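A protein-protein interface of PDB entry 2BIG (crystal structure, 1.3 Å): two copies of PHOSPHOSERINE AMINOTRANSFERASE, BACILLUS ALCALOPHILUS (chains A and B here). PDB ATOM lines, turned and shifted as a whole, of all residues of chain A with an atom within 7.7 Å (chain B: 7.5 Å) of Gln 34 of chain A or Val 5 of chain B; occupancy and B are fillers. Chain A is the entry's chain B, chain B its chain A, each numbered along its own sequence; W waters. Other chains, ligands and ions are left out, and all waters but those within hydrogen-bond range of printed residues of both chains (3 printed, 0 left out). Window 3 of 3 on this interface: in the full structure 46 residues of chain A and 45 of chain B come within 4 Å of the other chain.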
ATOM      1  N   LEU A  27      28.312   1.234 -16.192  1.00  0.00           N
ATOM      2  CA  LEU A  27      27.803   2.535 -16.610  1.00  0.00           C
ATOM      3  C   LEU A  27      27.742   2.659 -18.116  1.00  0.00           C
ATOM      4  O   LEU A  27      26.887   3.421 -18.623  1.00  0.00           O
ATOM      5  CB  LEU A  27      28.662   3.670 -16.002  1.00  0.00           C
ATOM      6  CG  LEU A  27      27.921   5.011 -15.924  1.00  0.00           C
ATOM      7  CD1 LEU A  27      26.871   4.971 -14.811  1.00  0.00           C
ATOM      8  CD2 LEU A  27      28.883   6.145 -15.691  1.00  0.00           C
ATOM      9  N   LEU A  28      28.634   2.004 -18.877  1.00  0.00           N
ATOM     10  CA  LEU A  28      28.661   2.162 -20.328  1.00  0.00           C
ATOM     11  C   LEU A  28      27.921   1.046 -21.049  1.00  0.00           C
ATOM     12  O   LEU A  28      27.527   1.195 -22.196  1.00  0.00           O
ATOM     13  CB  LEU A  28      30.108   2.178 -20.846  1.00  0.00           C
ATOM     14  CG  LEU A  28      31.110   3.078 -20.126  1.00  0.00           C
ATOM     15  CD1 LEU A  28      32.454   2.989 -20.855  1.00  0.00           C
ATOM     16  CD2 LEU A  28      30.610   4.491 -20.084  1.00  0.00           C
ATOM     17  N   ASN A  29      27.775  -0.092 -20.355  1.00  0.00           N
ATOM     18  CA  ASN A  29      27.163  -1.285 -20.949  1.00  0.00           C
ATOM     19  C   ASN A  29      26.288  -1.985 -19.916  1.00  0.00           C
ATOM     20  O   ASN A  29      26.741  -2.838 -19.152  1.00  0.00           O
ATOM     21  CB  ASN A  29      28.239  -2.230 -21.451  1.00  0.00           C
ATOM     22  CG  ASN A  29      27.710  -3.506 -22.037  1.00  0.00           C
ATOM     23  OD1 ASN A  29      26.532  -3.602 -22.333  1.00  0.00           O
ATOM     24  ND2 ASN A  29      28.595  -4.474 -22.235  1.00  0.00           N
ATOM     25  N   PHE A  30      25.031  -1.583 -19.870  1.00  0.00           N
ATOM     26  CA  PHE A  30      24.030  -2.177 -18.945  1.00  0.00           C
ATOM     27  C   PHE A  30      23.399  -3.401 -19.549  1.00  0.00           C
ATOM     28  O   PHE A  30      22.855  -3.325 -20.651  1.00  0.00           O
ATOM     29  CB  PHE A  30      22.974  -1.098 -18.666  1.00  0.00           C
ATOM     30  CG  PHE A  30      21.812  -1.679 -17.878  1.00  0.00           C
ATOM     31  CD1 PHE A  30      21.964  -1.970 -16.517  1.00  0.00           C
ATOM     32  CD2 PHE A  30      20.611  -1.937 -18.472  1.00  0.00           C
ATOM     33  CE1 PHE A  30      20.924  -2.549 -15.797  1.00  0.00           C
ATOM     34  CE2 PHE A  30      19.574  -2.525 -17.766  1.00  0.00           C
ATOM     35  CZ  PHE A  30      19.721  -2.818 -16.434  1.00  0.00           C
ATOM     36  N   ASN A  31      23.461  -4.530 -18.834  1.00  0.00           N
ATOM     37  CA  ASN A  31      22.769  -5.741 -19.208  1.00  0.00           C
ATOM     38  C   ASN A  31      23.012  -6.170 -20.647  1.00  0.00           C
ATOM     39  O   ASN A  31      22.072  -6.602 -21.305  1.00  0.00           O
ATOM     40  CB  ASN A  31      21.266  -5.526 -18.999  1.00  0.00           C
ATOM     41  CG  ASN A  31      20.486  -6.811 -18.804  1.00  0.00           C
ATOM     42  OD1 ASN A  31      21.064  -7.858 -18.505  1.00  0.00           O
ATOM     43  ND2 ASN A  31      19.181  -6.677 -19.013  1.00  0.00           N
ATOM     44  N   ASP A  32      24.262  -6.067 -21.078  1.00  0.00           N
ATOM     45  CA  ASP A  32      24.780  -6.449 -22.364  1.00  0.00           C
ATOM     46  C   ASP A  32      24.106  -5.720 -23.507  1.00  0.00           C
ATOM     47  O   ASP A  32      24.152  -6.182 -24.661  1.00  0.00           O
ATOM     48  CB  ASP A  32      24.638  -7.974 -22.591  1.00  0.00           C
ATOM     49  CG  ASP A  32      25.386  -8.763 -21.545  1.00  0.00           C
ATOM     50  OD1 ASP A  32      26.597  -8.477 -21.449  1.00  0.00           O
ATOM     51  OD2 ASP A  32      24.793  -9.647 -20.863  1.00  0.00           O
ATOM     52  N   THR A  33      23.484  -4.553 -23.261  1.00  0.00           N
ATOM     53  CA  THR A  33      22.842  -3.799 -24.323  1.00  0.00           C
ATOM     54  C   THR A  33      23.834  -2.915 -25.063  1.00  0.00           C
ATOM     55  O   THR A  33      23.448  -2.378 -26.105  1.00  0.00           O
ATOM     56  CB  THR A  33      21.745  -2.848 -23.797  1.00  0.00           C
ATOM     57  OG1 THR A  33      22.347  -1.844 -22.974  1.00  0.00           O
ATOM     58  CG2 THR A  33      20.694  -3.616 -23.004  1.00  0.00           C
ATOM     59  N   GLN A  34      25.025  -2.710 -24.552  1.00  0.00           N
ATOM     60  CA  GLN A  34      26.039  -1.795 -25.082  1.00  0.00           C
ATOM     61  C   GLN A  34      25.610  -0.331 -24.964  1.00  0.00           C
ATOM     62  O   GLN A  34      26.212   0.558 -25.586  1.00  0.00           O
ATOM     63  CB  GLN A  34      26.463  -2.154 -26.524  1.00  0.00           C
ATOM     64  CG  GLN A  34      26.947  -3.577 -26.617  1.00  0.00           C
ATOM     65  CD  GLN A  34      28.211  -3.846 -25.834  1.00  0.00           C
ATOM     66  OE1 GLN A  34      28.985  -2.893 -25.585  1.00  0.00           O
ATOM     67  NE2 GLN A  34      28.427  -5.081 -25.416  1.00  0.00           N
ATOM     68  N   MET A  35      24.607  -0.088 -24.107  1.00  0.00           N
ATOM     69  CA  MET A  35      24.177   1.253 -23.760  1.00  0.00           C
ATOM     70  C   MET A  35      24.207   1.420 -22.254  1.00  0.00           C
ATOM     71  O   MET A  35      24.023   0.454 -21.504  1.00  0.00           O
ATOM     72  CB  MET A  35      22.728   1.510 -24.225  1.00  0.00           C
ATOM     73  CG  MET A  35      22.569   1.511 -25.710  1.00  0.00           C
ATOM     74  SD  MET A  35      20.868   1.578 -26.281  1.00  0.00           S
ATOM     75  CE  MET A  35      20.384  -0.107 -25.958  1.00  0.00           C
ATOM     76  N   SER A  36      24.401   2.635 -21.776  1.00  0.00           N
ATOM     77  CA  SER A  36      24.197   2.935 -20.383  1.00  0.00           C
ATOM     78  C   SER A  36      22.728   2.832 -20.049  1.00  0.00           C
ATOM     79  O   SER A  36      21.854   3.080 -20.914  1.00  0.00           O
ATOM     80  CB  SER A  36      24.610   4.404 -20.139  1.00  0.00           C
ATOM     81  OG  SER A  36      24.476   4.752 -18.764  1.00  0.00           O
ATOM     82  N   VAL A  37      22.417   2.566 -18.792  1.00  0.00           N
ATOM     83  CA  VAL A  37      21.012   2.635 -18.375  1.00  0.00           C
ATOM     84  C   VAL A  37      20.465   4.024 -18.679  1.00  0.00           C
ATOM     85  O   VAL A  37      19.262   4.166 -18.962  1.00  0.00           O
ATOM     86  CB  VAL A  37      20.914   2.190 -16.883  1.00  0.00           C
ATOM     87  CG1 VAL A  37      21.495   3.215 -15.974  1.00  0.00           C
ATOM     88  CG2 VAL A  37      19.465   1.908 -16.528  1.00  0.00           C
ATOM     89  N   GLU A  39      20.869   5.772 -21.334  1.00  0.00           N
ATOM     90  CA  GLU A  39      20.660   5.884 -22.776  1.00  0.00           C
ATOM     91  C   GLU A  39      19.518   5.040 -23.311  1.00  0.00           C
ATOM     92  O   GLU A  39      19.269   5.016 -24.531  1.00  0.00           O
ATOM     93  CB  GLU A  39      21.937   5.461 -23.486  1.00  0.00           C
ATOM     94  CG  GLU A  39      23.139   6.388 -23.260  1.00  0.00           C
ATOM     95  CD  GLU A  39      24.386   5.876 -23.953  1.00  0.00           C
ATOM     96  OE1 GLU A  39      24.898   4.786 -23.560  1.00  0.00           O
ATOM     97  OE2 GLU A  39      24.836   6.569 -24.894  1.00  0.00           O
ATOM     98  N   LEU A  40      18.820   4.363 -22.396  1.00  0.00           N
ATOM     99  CA  LEU A  40      17.679   3.526 -22.705  1.00  0.00           C
ATOM    100  C   LEU A  40      16.393   4.326 -22.793  1.00  0.00           C
ATOM    101  O   LEU A  40      16.160   5.191 -21.972  1.00  0.00           O
ATOM    102  CB  LEU A  40      17.464   2.455 -21.648  1.00  0.00           C
ATOM    103  CG  LEU A  40      18.603   1.503 -21.336  1.00  0.00           C
ATOM    104  CD1 LEU A  40      18.212   0.579 -20.194  1.00  0.00           C
ATOM    105  CD2 LEU A  40      18.981   0.660 -22.535  1.00  0.00           C
ATOM    106  N   GLN B   4      27.219  -5.291 -32.693  1.00  0.00           N
ATOM    107  CA  GLN B   4      26.969  -3.904 -33.108  1.00  0.00           C
ATOM    108  C   GLN B   4      25.622  -3.380 -32.620  1.00  0.00           C
ATOM    109  O   GLN B   4      24.604  -4.031 -32.761  1.00  0.00           O
ATOM    110  CB  GLN B   4      26.994  -3.645 -34.619  1.00  0.00           C
ATOM    111  CG  GLN B   4      27.725  -2.320 -34.846  1.00  0.00           C
ATOM    112  CD  GLN B   4      29.234  -2.470 -34.896  1.00  0.00           C
ATOM    113  OE1 GLN B   4      29.969  -1.498 -34.659  1.00  0.00           O
ATOM    114  NE2 GLN B   4      29.705  -3.678 -35.187  1.00  0.00           N
ATOM    115  N   VAL B   5      25.645  -2.184 -32.049  1.00  0.00           N
ATOM    116  CA  VAL B   5      24.450  -1.547 -31.520  1.00  0.00           C
ATOM    117  C   VAL B   5      24.385  -0.107 -32.029  1.00  0.00           C
ATOM    118  O   VAL B   5      25.366   0.614 -31.929  1.00  0.00           O
ATOM    119  CB  VAL B   5      24.450  -1.603 -29.992  1.00  0.00           C
ATOM    120  CG1 VAL B   5      23.335  -0.764 -29.441  1.00  0.00           C
ATOM    121  CG2 VAL B   5      24.351  -3.050 -29.514  1.00  0.00           C
ATOM    122  N   PHE B   6      23.246   0.255 -32.587  1.00  0.00           N
ATOM    123  CA  PHE B   6      23.026   1.588 -33.102  1.00  0.00           C
ATOM    124  C   PHE B   6      21.865   2.194 -32.359  1.00  0.00           C
ATOM    125  O   PHE B   6      20.725   1.722 -32.465  1.00  0.00           O
ATOM    126  CB  PHE B   6      22.726   1.533 -34.595  1.00  0.00           C
ATOM    127  CG  PHE B   6      23.776   0.772 -35.381  1.00  0.00           C
ATOM    128  CD1 PHE B   6      23.488  -0.499 -35.860  1.00  0.00           C
ATOM    129  CD2 PHE B   6      25.016   1.308 -35.648  1.00  0.00           C
ATOM    130  CE1 PHE B   6      24.404  -1.236 -36.576  1.00  0.00           C
ATOM    131  CE2 PHE B   6      25.970   0.590 -36.350  1.00  0.00           C
ATOM    132  CZ  PHE B   6      25.654  -0.692 -36.813  1.00  0.00           C
ATOM    133  N   ASN B   7      22.136   3.235 -31.575  1.00  0.00           N
ATOM    134  CA  ASN B   7      21.134   3.752 -30.646  1.00  0.00           C
ATOM    135  C   ASN B   7      20.369   4.963 -31.186  1.00  0.00           C
ATOM    136  O   ASN B   7      20.827   6.096 -31.116  1.00  0.00           O
ATOM    137  CB  ASN B   7      21.795   4.146 -29.326  1.00  0.00           C
ATOM    138  CG  ASN B   7      20.805   4.558 -28.261  1.00  0.00           C
ATOM    139  OD1 ASN B   7      19.593   4.568 -28.530  1.00  0.00           O
ATOM    140  ND2 ASN B   7      21.343   4.921 -27.076  1.00  0.00           N
ATOM    141  N   PHE B   8      19.210   4.668 -31.717  1.00  0.00           N
ATOM    142  CA  PHE B   8      18.273   5.654 -32.239  1.00  0.00           C
ATOM    143  C   PHE B   8      17.123   5.906 -31.280  1.00  0.00           C
ATOM    144  O   PHE B   8      16.055   6.353 -31.680  1.00  0.00           O
ATOM    145  CB  PHE B   8      17.757   5.235 -33.616  1.00  0.00           C
ATOM    146  CG  PHE B   8      18.782   5.314 -34.718  1.00  0.00           C
ATOM    147  CD1 PHE B   8      19.542   4.227 -35.074  1.00  0.00           C
ATOM    148  CD2 PHE B   8      18.976   6.495 -35.410  1.00  0.00           C
ATOM    149  CE1 PHE B   8      20.453   4.344 -36.114  1.00  0.00           C
ATOM    150  CE2 PHE B   8      19.891   6.628 -36.453  1.00  0.00           C
ATOM    151  CZ  PHE B   8      20.630   5.530 -36.790  1.00  0.00           C
ATOM    152  N   LYS B  17      29.863   9.558 -25.634  1.00  0.00           N
ATOM    153  CA  LYS B  17      30.683   8.662 -24.827  1.00  0.00           C
ATOM    154  C   LYS B  17      31.645   9.390 -23.887  1.00  0.00           C
ATOM    155  O   LYS B  17      31.764   8.916 -22.775  1.00  0.00           O
ATOM    156  CB  LYS B  17      31.427   7.670 -25.726  1.00  0.00           C
ATOM    157  CG  LYS B  17      30.660   6.410 -25.999  1.00  0.00           C
ATOM    158  CD  LYS B  17      30.617   5.363 -24.908  1.00  0.00           C
ATOM    159  CE  LYS B  17      29.796   4.170 -25.407  1.00  0.00           C
ATOM    160  NZ  LYS B  17      29.727   3.134 -24.348  1.00  0.00           N
ATOM    161  N   GLN B 320      19.622  -6.614 -36.545  1.00  0.00           N
ATOM    162  CA  GLN B 320      20.879  -6.046 -36.958  1.00  0.00           C
ATOM    163  C   GLN B 320      21.449  -5.083 -35.935  1.00  0.00           C
ATOM    164  O   GLN B 320      22.495  -4.487 -36.164  1.00  0.00           O
ATOM    165  CB  GLN B 320      20.666  -5.355 -38.319  1.00  0.00           C
ATOM    166  CG  GLN B 320      20.465  -6.346 -39.473  1.00  0.00           C
ATOM    167  CD  GLN B 320      21.703  -7.192 -39.688  1.00  0.00           C
ATOM    168  OE1 GLN B 320      21.614  -8.414 -39.574  1.00  0.00           O
ATOM    169  NE2 GLN B 320      22.841  -6.545 -39.971  1.00  0.00           N
ATOM    170  N   GLY B 321      20.817  -4.932 -34.769  1.00  0.00           N
ATOM    171  CA  GLY B 321      21.403  -4.127 -33.719  1.00  0.00           C
ATOM    172  C   GLY B 321      20.880  -2.718 -33.589  1.00  0.00           C
ATOM    173  O   GLY B 321      21.346  -2.001 -32.668  1.00  0.00           O
ATOM    174  N   PHE B 322      19.914  -2.332 -34.402  1.00  0.00           N
ATOM    175  CA  PHE B 322      19.327  -1.003 -34.278  1.00  0.00           C
ATOM    176  C   PHE B 322      18.281  -0.975 -33.152  1.00  0.00           C
ATOM    177  O   PHE B 322      17.445  -1.867 -33.048  1.00  0.00           O
ATOM    178  CB  PHE B 322      18.615  -0.646 -35.595  1.00  0.00           C
ATOM    179  CG  PHE B 322      19.598  -0.496 -36.713  1.00  0.00           C
ATOM    180  CD1 PHE B 322      20.046  -1.570 -37.440  1.00  0.00           C
ATOM    181  CD2 PHE B 322      20.099   0.764 -37.057  1.00  0.00           C
ATOM    182  CE1 PHE B 322      20.967  -1.395 -38.444  1.00  0.00           C
ATOM    183  CE2 PHE B 322      21.044   0.944 -38.047  1.00  0.00           C
ATOM    184  CZ  PHE B 322      21.456  -0.147 -38.748  1.00  0.00           C
ATOM    185  N   VAL B 323      18.354   0.060 -32.326  1.00  0.00           N
ATOM    186  CA  VAL B 323      17.535   0.272 -31.166  1.00  0.00           C
ATOM    187  C   VAL B 323      16.723   1.540 -31.351  1.00  0.00           C
ATOM    188  O   VAL B 323      17.264   2.576 -31.676  1.00  0.00           O
ATOM    189  CB  VAL B 323      18.408   0.377 -29.889  1.00  0.00           C
ATOM    190  CG1 VAL B 323      17.521   0.622 -28.675  1.00  0.00           C
ATOM    191  CG2 VAL B 323      19.260  -0.881 -29.698  1.00  0.00           C
ATOM    192  N   PRO B 343      26.037   9.074 -33.353  1.00  0.00           N
ATOM    193  CA  PRO B 343      27.188   9.202 -34.238  1.00  0.00           C
ATOM    194  C   PRO B 343      26.814   9.064 -35.714  1.00  0.00           C
ATOM    195  O   PRO B 343      25.890   8.377 -36.076  1.00  0.00           O
ATOM    196  CB  PRO B 343      28.121   8.062 -33.810  1.00  0.00           C
ATOM    197  CG  PRO B 343      27.263   7.108 -33.069  1.00  0.00           C
ATOM    198  CD  PRO B 343      26.067   7.868 -32.534  1.00  0.00           C
ATOM    199  N   ASP B 345      28.297   7.366 -37.924  1.00  0.00           N
ATOM    200  CA  ASP B 345      28.359   6.006 -38.482  1.00  0.00           C
ATOM    201  C   ASP B 345      27.088   5.232 -38.153  1.00  0.00           C
ATOM    202  O   ASP B 345      26.820   4.254 -38.888  1.00  0.00           O
ATOM    203  CB  ASP B 345      29.605   5.286 -38.043  1.00  0.00           C
ATOM    204  CG  ASP B 345      29.860   5.038 -36.592  1.00  0.00           C
ATOM    205  OD1 ASP B 345      29.021   5.462 -35.759  1.00  0.00           O
ATOM    206  OD2 ASP B 345      30.918   4.422 -36.247  1.00  0.00           O
ATOM    207  N   ALA B 346      26.295   5.633 -37.164  1.00  0.00           N
ATOM    208  CA  ALA B 346      25.018   4.952 -37.001  1.00  0.00           C
ATOM    209  C   ALA B 346      24.066   5.295 -38.150  1.00  0.00           C
ATOM    210  O   ALA B 346      23.267   4.472 -38.606  1.00  0.00           O
ATOM    211  CB  ALA B 346      24.414   5.310 -35.651  1.00  0.00           C
HETATM  212  O   HOH W   1      24.328   4.925 -27.069  1.00  0.00           O
HETATM  213  O   HOH W   2      27.476   3.696 -23.427  1.00  0.00           O
HETATM  214  O   HOH W   3      29.000   0.578 -24.614  1.00  0.00           O
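ND2 of Asn 7 of chain B sits at hydrogen-bond distance from SD of Met 35 of chain A (3.5 Å). The backbone carbonyl oxygen (O) of Glu 39 of chain A is in hydrogen-bond range of the side-chain amide nitrogen (ND2) of Asn 7 of chain B (3.3 Å).
The backbone NH (N) of Ser 36 of chain A is in hydrogen-bond range of the side-chain carboxylate (OE1) of Glu 39 of chain A, at 2.8 Å. The backbone carbonyl oxygen of Phe 30 of chain A sits at hydrogen-bond distance from the side-chain hydroxyl of Thr 33 of chain A, at 2.8 Å. The backbone NH (N) of Phe 8 of chain B lies within hydrogen-bond range of the backbone carbonyl oxygen (O) of Val 323 of chain B (2.9 Å). N of Phe 30 of chain A is in hydrogen-bond range of O of Met 35 of chain A, at 2.8 Å. OG1 of Thr 33 of chain A sits at hydrogen-bond distance from N of Met 35 of chain A (3.1 Å). The side-chain amide oxygen (OD1) of Asn 29 of chain A is in hydrogen-bond range of the backbone NH (N) of Gln 34 of chain A (2.8 Å).
Among the printed residues, merely in contact across the chains: Leu 28 of chain A with Lys 17 of chain B (3.6 Å), Thr 33 of chain A with Val 5 of chain B (3.6 Å), Gln 34 of chain A with Val 5 of chain B (3.8 Å) and Met 35 of chain A with Val 323 of chain B (3.98 Å).
Val 5 of chain B touches just these residues of chain A: Thr 33 and Gln 34. Of the printed residues of chain B, Glu 39 of chain A touches Asn 7 (3.3 Å). Of the printed residues of chain B, Thr 33 of chain A touches Val 5. The nearest residue of chain B that does not touch Gln 34 of chain A is Lys 17 of chain B (4.5 Å). The nearest printed residue of chain A that does not touch Lys 17 of chain B is Gln 34 of chain A (4.5 Å).
Along chain A the printed residues that touch a printed residue of chain B span positions 28 to 39. Of the 13 printed residues of chain B, 4 touch a printed residue of chain A. Hydrophobic or aromatic side chains of chain B within 4 Å of the printed part of chain A: Val 5 and Val 323. Among the printed residues, no Asp or Glu carboxylate lies within 4 Å of a Lys or Arg side-chain nitrogen of the other chain.
No position is printed for both chains. Of the 6 pairs that touch across the chains among the printed residues, none has its exchanged pair printed and touching as well.
Water W2 lies within hydrogen-bond range of NZ of Lys 17 of chain B (2.5 Å), O of Leu 28 of chain A (2.8 Å) and OE1 of Glu 39 of chain A (2.8 Å). Water W3 lies within hydrogen-bond range of the side-chain amino group (NZ) of Lys 17 of chain B (2.7 Å), the backbone carbonyl oxygen (O) of Leu 28 of chain A (2.9 Å) and the backbone carbonyl oxygen (O) of Gln 34 of chain A (3.0 Å). Water W1 lies within hydrogen-bond range of OE2 of Glu 39 of chain A and ND2 of Asn 7 of chain B.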
